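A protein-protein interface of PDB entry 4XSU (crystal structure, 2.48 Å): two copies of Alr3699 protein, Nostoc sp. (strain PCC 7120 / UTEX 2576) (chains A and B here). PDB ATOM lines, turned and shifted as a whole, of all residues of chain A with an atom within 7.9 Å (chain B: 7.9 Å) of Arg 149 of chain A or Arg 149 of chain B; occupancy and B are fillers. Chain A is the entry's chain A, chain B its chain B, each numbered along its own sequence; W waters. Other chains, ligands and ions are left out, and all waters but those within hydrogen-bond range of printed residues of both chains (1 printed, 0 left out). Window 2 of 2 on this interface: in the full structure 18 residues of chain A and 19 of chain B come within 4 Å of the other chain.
The guanidinium group of Arg 149 of chain A sits close to the guanidinium group of Arg 149 of chain B (3.1 Å).
Among the printed residues, merely in contact across the chains: Phe 116 of chain A with Asn 145 of chain B and Asn 145 of chain A with Phe 116 of chain B.
Of chain A, only Arg 149 comes within 4 Å of Arg 149 of chain B. Printed residues of chain B within 4 Å of Asn 145 of chain A: Phe 116. Of the printed residues of chain A, Phe 116 of chain B touches Asn 145. Val 144 of chain A touches none of the printed residues of chain B. The nearest residue of chain B that does not touch Arg 149 of chain A is Asn 145 of chain B (7.0 Å). The nearest residue of chain A that does not touch Arg 149 of chain B is Asn 145 of chain A (5.4 Å).
Of the 17 printed residues of chain A, 3 touch a printed residue of chain B. Hydrophobic or aromatic side chains of chain A that line the printed part of chain B: Phe 116. Hydrophobic or aromatic side chains of chain B within 4 Å of the printed part of chain A: Phe 116. Among the printed residues, 3 pairs touch across the chains. Among the printed residues, no Asp or Glu carboxylate lies within 4 Å of a Lys or Arg side-chain nitrogen of the other chain.
Phe 116 of chain A touches Asn 145 of chain B, and with the chains exchanged Asn 145 of chain A touches Phe 116 of chain B. Arg 149 of chain A touches its own counterpart, Arg 149 of chain B. Positions printed for both chains: 112, 115, 116, 122, 142, 143, 144, 145, 146, 147, 148, 149, 150, 151, 152, 171 and 174. Of the 3 pairs that touch across the chains among the printed residues, 3 have their exchanged pair printed and touching as well.
Water W1 bridges the guanidinium group (NE) of Arg 149 of chain A (2.7 Å) and the guanidinium group (NH2) of Arg 149 of chain B (3.4 Å).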
ATOM      1  N   ALA A 112       1.436 -21.248  -6.440  1.00  0.00           N
ATOM      2  CA  ALA A 112       2.211 -21.999  -5.458  1.00  0.00           C
ATOM      3  C   ALA A 112       1.291 -22.842  -4.519  1.00  0.00           C
ATOM      4  O   ALA A 112       1.418 -24.066  -4.374  1.00  0.00           O
ATOM      5  CB  ALA A 112       3.035 -21.039  -4.649  1.00  0.00           C
ATOM      6  N   SER A 115      -0.219 -25.444  -6.378  1.00  0.00           N
ATOM      7  CA  SER A 115       0.806 -26.421  -6.765  1.00  0.00           C
ATOM      8  C   SER A 115       0.965 -27.466  -5.647  1.00  0.00           C
ATOM      9  O   SER A 115       0.990 -28.669  -5.890  1.00  0.00           O
ATOM     10  CB  SER A 115       2.155 -25.731  -7.043  1.00  0.00           C
ATOM     11  OG  SER A 115       3.198 -26.680  -7.226  1.00  0.00           O
ATOM     12  N   PHE A 116       1.074 -26.980  -4.419  1.00  0.00           N
ATOM     13  CA  PHE A 116       1.274 -27.850  -3.266  1.00  0.00           C
ATOM     14  C   PHE A 116       0.064 -28.736  -2.970  1.00  0.00           C
ATOM     15  O   PHE A 116       0.167 -29.957  -2.847  1.00  0.00           O
ATOM     16  CB  PHE A 116       1.564 -27.019  -2.032  1.00  0.00           C
ATOM     17  CG  PHE A 116       1.737 -27.840  -0.809  1.00  0.00           C
ATOM     18  CD1 PHE A 116       2.873 -28.604  -0.643  1.00  0.00           C
ATOM     19  CD2 PHE A 116       0.749 -27.886   0.151  1.00  0.00           C
ATOM     20  CE1 PHE A 116       3.038 -29.380   0.479  1.00  0.00           C
ATOM     21  CE2 PHE A 116       0.909 -28.658   1.273  1.00  0.00           C
ATOM     22  CZ  PHE A 116       2.052 -29.405   1.434  1.00  0.00           C
ATOM     23  N   LEU A 122       4.725 -26.465 -11.126  1.00  0.00           N
ATOM     24  CA  LEU A 122       4.450 -25.061 -11.311  1.00  0.00           C
ATOM     25  C   LEU A 122       5.575 -24.423 -12.104  1.00  0.00           C
ATOM     26  O   LEU A 122       6.773 -24.628 -11.794  1.00  0.00           O
ATOM     27  CB  LEU A 122       4.355 -24.362  -9.962  1.00  0.00           C
ATOM     28  CG  LEU A 122       4.364 -22.822  -9.921  1.00  0.00           C
ATOM     29  CD1 LEU A 122       3.004 -22.230 -10.282  1.00  0.00           C
ATOM     30  CD2 LEU A 122       4.801 -22.340  -8.537  1.00  0.00           C
ATOM     31  N   VAL A 142       8.545 -12.534  -1.157  1.00  0.00           N
ATOM     32  CA  VAL A 142       7.536 -13.544  -1.401  1.00  0.00           C
ATOM     33  C   VAL A 142       7.801 -14.288  -2.690  1.00  0.00           C
ATOM     34  O   VAL A 142       7.816 -15.527  -2.711  1.00  0.00           O
ATOM     35  CB  VAL A 142       6.141 -12.926  -1.448  1.00  0.00           C
ATOM     36  CG1 VAL A 142       5.109 -13.942  -1.926  1.00  0.00           C
ATOM     37  CG2 VAL A 142       5.773 -12.366  -0.085  1.00  0.00           C
ATOM     38  N   ALA A 143       7.984 -13.527  -3.776  1.00  0.00           N
ATOM     39  CA  ALA A 143       8.168 -14.091  -5.123  1.00  0.00           C
ATOM     40  C   ALA A 143       9.392 -14.995  -5.178  1.00  0.00           C
ATOM     41  O   ALA A 143       9.345 -16.098  -5.668  1.00  0.00           O
ATOM     42  CB  ALA A 143       8.293 -12.954  -6.127  1.00  0.00           C
ATOM     43  N   VAL A 144      10.492 -14.533  -4.635  1.00  0.00           N
ATOM     44  CA  VAL A 144      11.715 -15.347  -4.588  1.00  0.00           C
ATOM     45  C   VAL A 144      11.541 -16.668  -3.803  1.00  0.00           C
ATOM     46  O   VAL A 144      11.895 -17.787  -4.282  1.00  0.00           O
ATOM     47  CB  VAL A 144      12.840 -14.504  -3.970  1.00  0.00           C
ATOM     48  CG1 VAL A 144      14.043 -15.360  -3.613  1.00  0.00           C
ATOM     49  CG2 VAL A 144      13.227 -13.384  -4.931  1.00  0.00           C
ATOM     50  N   ASN A 145      10.986 -16.550  -2.596  1.00  0.00           N
ATOM     51  CA  ASN A 145      10.794 -17.736  -1.757  1.00  0.00           C
ATOM     52  C   ASN A 145       9.816 -18.708  -2.367  1.00  0.00           C
ATOM     53  O   ASN A 145      10.107 -19.900  -2.440  1.00  0.00           O
ATOM     54  CB  ASN A 145      10.421 -17.351  -0.330  1.00  0.00           C
ATOM     55  CG  ASN A 145      11.620 -16.850   0.451  1.00  0.00           C
ATOM     56  OD1 ASN A 145      12.288 -17.627   1.106  1.00  0.00           O
ATOM     57  ND2 ASN A 145      11.934 -15.571   0.333  1.00  0.00           N
ATOM     58  N   LEU A 146       8.684 -18.212  -2.855  1.00  0.00           N
ATOM     59  CA  LEU A 146       7.703 -19.098  -3.487  1.00  0.00           C
ATOM     60  C   LEU A 146       8.238 -19.748  -4.768  1.00  0.00           C
ATOM     61  O   LEU A 146       7.974 -20.938  -5.044  1.00  0.00           O
ATOM     62  CB  LEU A 146       6.404 -18.353  -3.790  1.00  0.00           C
ATOM     63  CG  LEU A 146       5.616 -17.861  -2.569  1.00  0.00           C
ATOM     64  CD1 LEU A 146       4.441 -16.992  -3.008  1.00  0.00           C
ATOM     65  CD2 LEU A 146       5.139 -19.036  -1.734  1.00  0.00           C
ATOM     66  N   ALA A 147       8.998 -18.984  -5.548  1.00  0.00           N
ATOM     67  CA  ALA A 147       9.578 -19.522  -6.771  1.00  0.00           C
ATOM     68  C   ALA A 147      10.596 -20.576  -6.405  1.00  0.00           C
ATOM     69  O   ALA A 147      10.511 -21.724  -6.876  1.00  0.00           O
ATOM     70  CB  ALA A 147      10.234 -18.413  -7.578  1.00  0.00           C
ATOM     71  N   ASN A 148      11.552 -20.180  -5.557  1.00  0.00           N
ATOM     72  CA  ASN A 148      12.601 -21.112  -5.102  1.00  0.00           C
ATOM     73  C   ASN A 148      12.051 -22.426  -4.547  1.00  0.00           C
ATOM     74  O   ASN A 148      12.520 -23.501  -4.926  1.00  0.00           O
ATOM     75  CB  ASN A 148      13.521 -20.441  -4.094  1.00  0.00           C
ATOM     76  CG  ASN A 148      14.477 -19.466  -4.757  1.00  0.00           C
ATOM     77  OD1 ASN A 148      14.579 -19.432  -5.974  1.00  0.00           O
ATOM     78  ND2 ASN A 148      15.167 -18.665  -3.966  1.00  0.00           N
ATOM     79  N   ARG A 149      10.994 -22.342  -3.737  1.00  0.00           N
ATOM     80  CA  ARG A 149      10.435 -23.519  -3.110  1.00  0.00           C
ATOM     81  C   ARG A 149       9.514 -24.294  -4.015  1.00  0.00           C
ATOM     82  O   ARG A 149       9.590 -25.520  -4.034  1.00  0.00           O
ATOM     83  CB  ARG A 149       9.707 -23.158  -1.818  1.00  0.00           C
ATOM     84  CG  ARG A 149       9.017 -24.343  -1.134  1.00  0.00           C
ATOM     85  CD  ARG A 149      10.000 -25.332  -0.503  1.00  0.00           C
ATOM     86  NE  ARG A 149      10.142 -25.126   0.940  1.00  0.00           N
ATOM     87  CZ  ARG A 149      10.373 -26.085   1.835  1.00  0.00           C
ATOM     88  NH1 ARG A 149      10.487 -27.358   1.463  1.00  0.00           N
ATOM     89  NH2 ARG A 149      10.481 -25.766   3.122  1.00  0.00           N
ATOM     90  N   PHE A 150       8.637 -23.618  -4.759  1.00  0.00           N
ATOM     91  CA  PHE A 150       7.585 -24.338  -5.510  1.00  0.00           C
ATOM     92  C   PHE A 150       7.712 -24.425  -7.048  1.00  0.00           C
ATOM     93  O   PHE A 150       7.038 -25.254  -7.692  1.00  0.00           O
ATOM     94  CB  PHE A 150       6.224 -23.740  -5.173  1.00  0.00           C
ATOM     95  CG  PHE A 150       5.896 -23.777  -3.717  1.00  0.00           C
ATOM     96  CD1 PHE A 150       5.326 -24.909  -3.151  1.00  0.00           C
ATOM     97  CD2 PHE A 150       6.157 -22.681  -2.914  1.00  0.00           C
ATOM     98  CE1 PHE A 150       5.033 -24.939  -1.800  1.00  0.00           C
ATOM     99  CE2 PHE A 150       5.865 -22.700  -1.570  1.00  0.00           C
ATOM    100  CZ  PHE A 150       5.304 -23.829  -1.008  1.00  0.00           C
ATOM    101  N   ALA A 151       8.535 -23.568  -7.649  1.00  0.00           N
ATOM    102  CA  ALA A 151       8.594 -23.514  -9.105  1.00  0.00           C
ATOM    103  C   ALA A 151       9.539 -24.565  -9.653  1.00  0.00           C
ATOM    104  O   ALA A 151      10.699 -24.590  -9.277  1.00  0.00           O
ATOM    105  CB  ALA A 151       9.029 -22.131  -9.541  1.00  0.00           C
ATOM    106  N   SER A 152       9.066 -25.433 -10.536  1.00  0.00           N
ATOM    107  CA  SER A 152       9.997 -26.272 -11.310  1.00  0.00           C
ATOM    108  C   SER A 152      10.915 -25.432 -12.217  1.00  0.00           C
ATOM    109  O   SER A 152      12.051 -25.821 -12.487  1.00  0.00           O
ATOM    110  CB  SER A 152       9.258 -27.299 -12.163  1.00  0.00           C
ATOM    111  OG  SER A 152       8.554 -28.222 -11.346  1.00  0.00           O
ATOM    112  N   ARG A 171      16.909 -18.566  -7.337  1.00  0.00           N
ATOM    113  CA  ARG A 171      17.829 -19.642  -7.677  1.00  0.00           C
ATOM    114  C   ARG A 171      18.150 -19.671  -9.171  1.00  0.00           C
ATOM    115  O   ARG A 171      17.369 -20.170 -10.014  1.00  0.00           O
ATOM    116  CB  ARG A 171      17.297 -21.007  -7.224  1.00  0.00           C
ATOM    117  CG  ARG A 171      17.687 -21.414  -5.791  1.00  0.00           C
ATOM    118  CD  ARG A 171      16.788 -22.544  -5.291  1.00  0.00           C
ATOM    119  NE  ARG A 171      17.067 -23.789  -6.009  1.00  0.00           N
ATOM    120  CZ  ARG A 171      16.185 -24.757  -6.276  1.00  0.00           C
ATOM    121  NH1 ARG A 171      14.917 -24.660  -5.914  1.00  0.00           N
ATOM    122  NH2 ARG A 171      16.575 -25.841  -6.936  1.00  0.00           N
ATOM    123  N   LEU A 174      17.187 -22.397 -11.645  1.00  0.00           N
ATOM    124  CA  LEU A 174      15.784 -22.531 -12.073  1.00  0.00           C
ATOM    125  C   LEU A 174      15.499 -21.676 -13.315  1.00  0.00           C
ATOM    126  O   LEU A 174      14.551 -21.931 -14.053  1.00  0.00           O
ATOM    127  CB  LEU A 174      14.826 -22.105 -10.940  1.00  0.00           C
ATOM    128  CG  LEU A 174      14.680 -23.066  -9.748  1.00  0.00           C
ATOM    129  CD1 LEU A 174      13.832 -22.420  -8.668  1.00  0.00           C
ATOM    130  CD2 LEU A 174      14.066 -24.397 -10.171  1.00  0.00           C
ATOM    131  N   ALA B 112       1.500 -18.188  10.414  1.00  0.00           N
ATOM    132  CA  ALA B 112       2.672 -18.608   9.651  1.00  0.00           C
ATOM    133  C   ALA B 112       3.078 -17.503   8.636  1.00  0.00           C
ATOM    134  O   ALA B 112       4.252 -17.132   8.518  1.00  0.00           O
ATOM    135  CB  ALA B 112       2.389 -19.913   8.936  1.00  0.00           C
ATOM    136  N   SER B 115       4.415 -14.593  10.420  1.00  0.00           N
ATOM    137  CA  SER B 115       5.694 -14.916  11.021  1.00  0.00           C
ATOM    138  C   SER B 115       6.810 -14.666  10.012  1.00  0.00           C
ATOM    139  O   SER B 115       7.805 -14.005  10.310  1.00  0.00           O
ATOM    140  CB  SER B 115       5.707 -16.384  11.452  1.00  0.00           C
ATOM    141  OG  SER B 115       6.977 -16.765  11.931  1.00  0.00           O
ATOM    142  N   PHE B 116       6.640 -15.211   8.813  1.00  0.00           N
ATOM    143  CA  PHE B 116       7.608 -15.012   7.732  1.00  0.00           C
ATOM    144  C   PHE B 116       7.847 -13.539   7.382  1.00  0.00           C
ATOM    145  O   PHE B 116       8.952 -13.036   7.423  1.00  0.00           O
ATOM    146  CB  PHE B 116       7.130 -15.715   6.471  1.00  0.00           C
ATOM    147  CG  PHE B 116       8.075 -15.561   5.331  1.00  0.00           C
ATOM    148  CD1 PHE B 116       9.239 -16.317   5.275  1.00  0.00           C
ATOM    149  CD2 PHE B 116       7.838 -14.622   4.347  1.00  0.00           C
ATOM    150  CE1 PHE B 116      10.138 -16.154   4.235  1.00  0.00           C
ATOM    151  CE2 PHE B 116       8.731 -14.461   3.308  1.00  0.00           C
ATOM    152  CZ  PHE B 116       9.880 -15.228   3.254  1.00  0.00           C
ATOM    153  N   LEU B 122       6.954 -18.091  15.853  1.00  0.00           N
ATOM    154  CA  LEU B 122       5.590 -18.537  15.883  1.00  0.00           C
ATOM    155  C   LEU B 122       5.481 -19.693  16.852  1.00  0.00           C
ATOM    156  O   LEU B 122       6.335 -20.611  16.846  1.00  0.00           O
ATOM    157  CB  LEU B 122       5.160 -19.003  14.501  1.00  0.00           C
ATOM    158  CG  LEU B 122       3.774 -19.627  14.389  1.00  0.00           C
ATOM    159  CD1 LEU B 122       2.688 -18.576  14.485  1.00  0.00           C
ATOM    160  CD2 LEU B 122       3.650 -20.382  13.082  1.00  0.00           C
ATOM    161  N   VAL B 142      -1.881 -29.132   5.423  1.00  0.00           N
ATOM    162  CA  VAL B 142      -1.530 -27.744   5.655  1.00  0.00           C
ATOM    163  C   VAL B 142      -0.962 -27.493   7.044  1.00  0.00           C
ATOM    164  O   VAL B 142       0.097 -26.837   7.189  1.00  0.00           O
ATOM    165  CB  VAL B 142      -2.722 -26.801   5.387  1.00  0.00           C
ATOM    166  CG1 VAL B 142      -2.399 -25.376   5.821  1.00  0.00           C
ATOM    167  CG2 VAL B 142      -3.074 -26.821   3.903  1.00  0.00           C
ATOM    168  N   ALA B 143      -1.664 -27.965   8.079  1.00  0.00           N
ATOM    169  CA  ALA B 143      -1.257 -27.642   9.457  1.00  0.00           C
ATOM    170  C   ALA B 143       0.138 -28.194   9.746  1.00  0.00           C
ATOM    171  O   ALA B 143       1.035 -27.497  10.237  1.00  0.00           O
ATOM    172  CB  ALA B 143      -2.276 -28.185  10.446  1.00  0.00           C
ATOM    173  N   VAL B 144       0.335 -29.443   9.379  1.00  0.00           N
ATOM    174  CA  VAL B 144       1.625 -30.105   9.609  1.00  0.00           C
ATOM    175  C   VAL B 144       2.771 -29.389   8.893  1.00  0.00           C
ATOM    176  O   VAL B 144       3.822 -29.092   9.491  1.00  0.00           O
ATOM    177  CB  VAL B 144       1.553 -31.532   9.078  1.00  0.00           C
ATOM    178  CG1 VAL B 144       2.944 -32.147   8.988  1.00  0.00           C
ATOM    179  CG2 VAL B 144       0.622 -32.357   9.948  1.00  0.00           C
ATOM    180  N   ASN B 145       2.569 -29.114   7.598  1.00  0.00           N
ATOM    181  CA  ASN B 145       3.582 -28.395   6.816  1.00  0.00           C
ATOM    182  C   ASN B 145       3.851 -27.002   7.337  1.00  0.00           C
ATOM    183  O   ASN B 145       5.013 -26.640   7.529  1.00  0.00           O
ATOM    184  CB  ASN B 145       3.238 -28.403   5.336  1.00  0.00           C
ATOM    185  CG  ASN B 145       3.547 -29.727   4.707  1.00  0.00           C
ATOM    186  OD1 ASN B 145       4.680 -29.985   4.317  1.00  0.00           O
ATOM    187  ND2 ASN B 145       2.562 -30.603   4.663  1.00  0.00           N
ATOM    188  N   LEU B 146       2.818 -26.230   7.653  1.00  0.00           N
ATOM    189  CA  LEU B 146       3.105 -24.885   8.191  1.00  0.00           C
ATOM    190  C   LEU B 146       3.760 -24.962   9.561  1.00  0.00           C
ATOM    191  O   LEU B 146       4.615 -24.132   9.900  1.00  0.00           O
ATOM    192  CB  LEU B 146       1.845 -24.018   8.276  1.00  0.00           C
ATOM    193  CG  LEU B 146       1.176 -23.754   6.927  1.00  0.00           C
ATOM    194  CD1 LEU B 146      -0.151 -23.043   7.089  1.00  0.00           C
ATOM    195  CD2 LEU B 146       2.106 -22.932   6.064  1.00  0.00           C
ATOM    196  N   ALA B 147       3.350 -25.945  10.363  1.00  0.00           N
ATOM    197  CA  ALA B 147       3.888 -26.061  11.718  1.00  0.00           C
ATOM    198  C   ALA B 147       5.349 -26.445  11.610  1.00  0.00           C
ATOM    199  O   ALA B 147       6.229 -25.768  12.157  1.00  0.00           O
ATOM    200  CB  ALA B 147       3.117 -27.096  12.509  1.00  0.00           C
ATOM    201  N   ASN B 148       5.602 -27.513  10.859  1.00  0.00           N
ATOM    202  CA  ASN B 148       6.986 -27.969  10.655  1.00  0.00           C
ATOM    203  C   ASN B 148       7.919 -26.879  10.189  1.00  0.00           C
ATOM    204  O   ASN B 148       9.032 -26.767  10.685  1.00  0.00           O
ATOM    205  CB  ASN B 148       7.036 -29.177   9.712  1.00  0.00           C
ATOM    206  CG  ASN B 148       6.548 -30.442  10.395  1.00  0.00           C
ATOM    207  OD1 ASN B 148       6.415 -30.461  11.606  1.00  0.00           O
ATOM    208  ND2 ASN B 148       6.267 -31.485   9.635  1.00  0.00           N
ATOM    209  N   ARG B 149       7.422 -26.018   9.311  1.00  0.00           N
ATOM    210  CA  ARG B 149       8.257 -25.049   8.655  1.00  0.00           C
ATOM    211  C   ARG B 149       8.381 -23.793   9.464  1.00  0.00           C
ATOM    212  O   ARG B 149       9.453 -23.237   9.552  1.00  0.00           O
ATOM    213  CB  ARG B 149       7.695 -24.749   7.251  1.00  0.00           C
ATOM    214  CG  ARG B 149       8.402 -23.630   6.477  1.00  0.00           C
ATOM    215  CD  ARG B 149       9.828 -23.986   6.081  1.00  0.00           C
ATOM    216  NE  ARG B 149      10.553 -22.841   5.520  1.00  0.00           N
ATOM    217  CZ  ARG B 149      11.759 -22.903   4.953  1.00  0.00           C
ATOM    218  NH1 ARG B 149      12.319 -21.796   4.480  1.00  0.00           N
ATOM    219  NH2 ARG B 149      12.413 -24.061   4.848  1.00  0.00           N
ATOM    220  N   PHE B 150       7.296 -23.308  10.045  1.00  0.00           N
ATOM    221  CA  PHE B 150       7.346 -21.974  10.675  1.00  0.00           C
ATOM    222  C   PHE B 150       7.290 -21.936  12.211  1.00  0.00           C
ATOM    223  O   PHE B 150       7.689 -20.938  12.823  1.00  0.00           O
ATOM    224  CB  PHE B 150       6.228 -21.106  10.119  1.00  0.00           C
ATOM    225  CG  PHE B 150       6.298 -20.925   8.645  1.00  0.00           C
ATOM    226  CD1 PHE B 150       7.129 -19.964   8.102  1.00  0.00           C
ATOM    227  CD2 PHE B 150       5.541 -21.728   7.797  1.00  0.00           C
ATOM    228  CE1 PHE B 150       7.199 -19.799   6.739  1.00  0.00           C
ATOM    229  CE2 PHE B 150       5.603 -21.565   6.431  1.00  0.00           C
ATOM    230  CZ  PHE B 150       6.433 -20.598   5.902  1.00  0.00           C
ATOM    231  N   ALA B 151       6.786 -22.997  12.833  1.00  0.00           N
ATOM    232  CA  ALA B 151       6.539 -22.954  14.259  1.00  0.00           C
ATOM    233  C   ALA B 151       7.805 -23.285  15.014  1.00  0.00           C
ATOM    234  O   ALA B 151       8.366 -24.363  14.810  1.00  0.00           O
ATOM    235  CB  ALA B 151       5.430 -23.921  14.615  1.00  0.00           C
ATOM    236  N   SER B 152       8.255 -22.375  15.878  1.00  0.00           N
ATOM    237  CA  SER B 152       9.348 -22.689  16.825  1.00  0.00           C
ATOM    238  C   SER B 152       8.942 -23.718  17.883  1.00  0.00           C
ATOM    239  O   SER B 152       9.796 -24.332  18.508  1.00  0.00           O
ATOM    240  CB  SER B 152       9.828 -21.446  17.559  1.00  0.00           C
ATOM    241  OG  SER B 152      10.198 -20.410  16.662  1.00  0.00           O
ATOM    242  N   ARG B 171       6.603 -32.807  13.317  1.00  0.00           N
ATOM    243  CA  ARG B 171       7.929 -33.000  13.804  1.00  0.00           C
ATOM    244  C   ARG B 171       7.876 -33.222  15.311  1.00  0.00           C
ATOM    245  O   ARG B 171       7.772 -32.273  16.102  1.00  0.00           O
ATOM    246  CB  ARG B 171       8.833 -31.811  13.429  1.00  0.00           C
ATOM    247  CG  ARG B 171       9.546 -31.999  12.071  1.00  0.00           C
ATOM    248  CD  ARG B 171      10.255 -30.729  11.588  1.00  0.00           C
ATOM    249  NE  ARG B 171      11.366 -30.375  12.465  1.00  0.00           N
ATOM    250  CZ  ARG B 171      11.743 -29.132  12.767  1.00  0.00           C
ATOM    251  NH1 ARG B 171      12.785 -28.933  13.586  1.00  0.00           N
ATOM    252  NH2 ARG B 171      11.089 -28.082  12.275  1.00  0.00           N
ATOM    253  N   LEU B 174       9.348 -30.700  17.832  1.00  0.00           N
ATOM    254  CA  LEU B 174       8.710 -29.402  18.067  1.00  0.00           C
ATOM    255  C   LEU B 174       7.654 -29.460  19.221  1.00  0.00           C
ATOM    256  O   LEU B 174       7.366 -28.436  19.872  1.00  0.00           O
ATOM    257  CB  LEU B 174       8.055 -28.901  16.772  1.00  0.00           C
ATOM    258  CG  LEU B 174       8.992 -28.472  15.630  1.00  0.00           C
ATOM    259  CD1 LEU B 174       8.159 -28.173  14.393  1.00  0.00           C
ATOM    260  CD2 LEU B 174       9.840 -27.264  16.011  1.00  0.00           C
HETATM  261  O   HOH W   1      12.449 -23.845   1.412  1.00  0.00           O
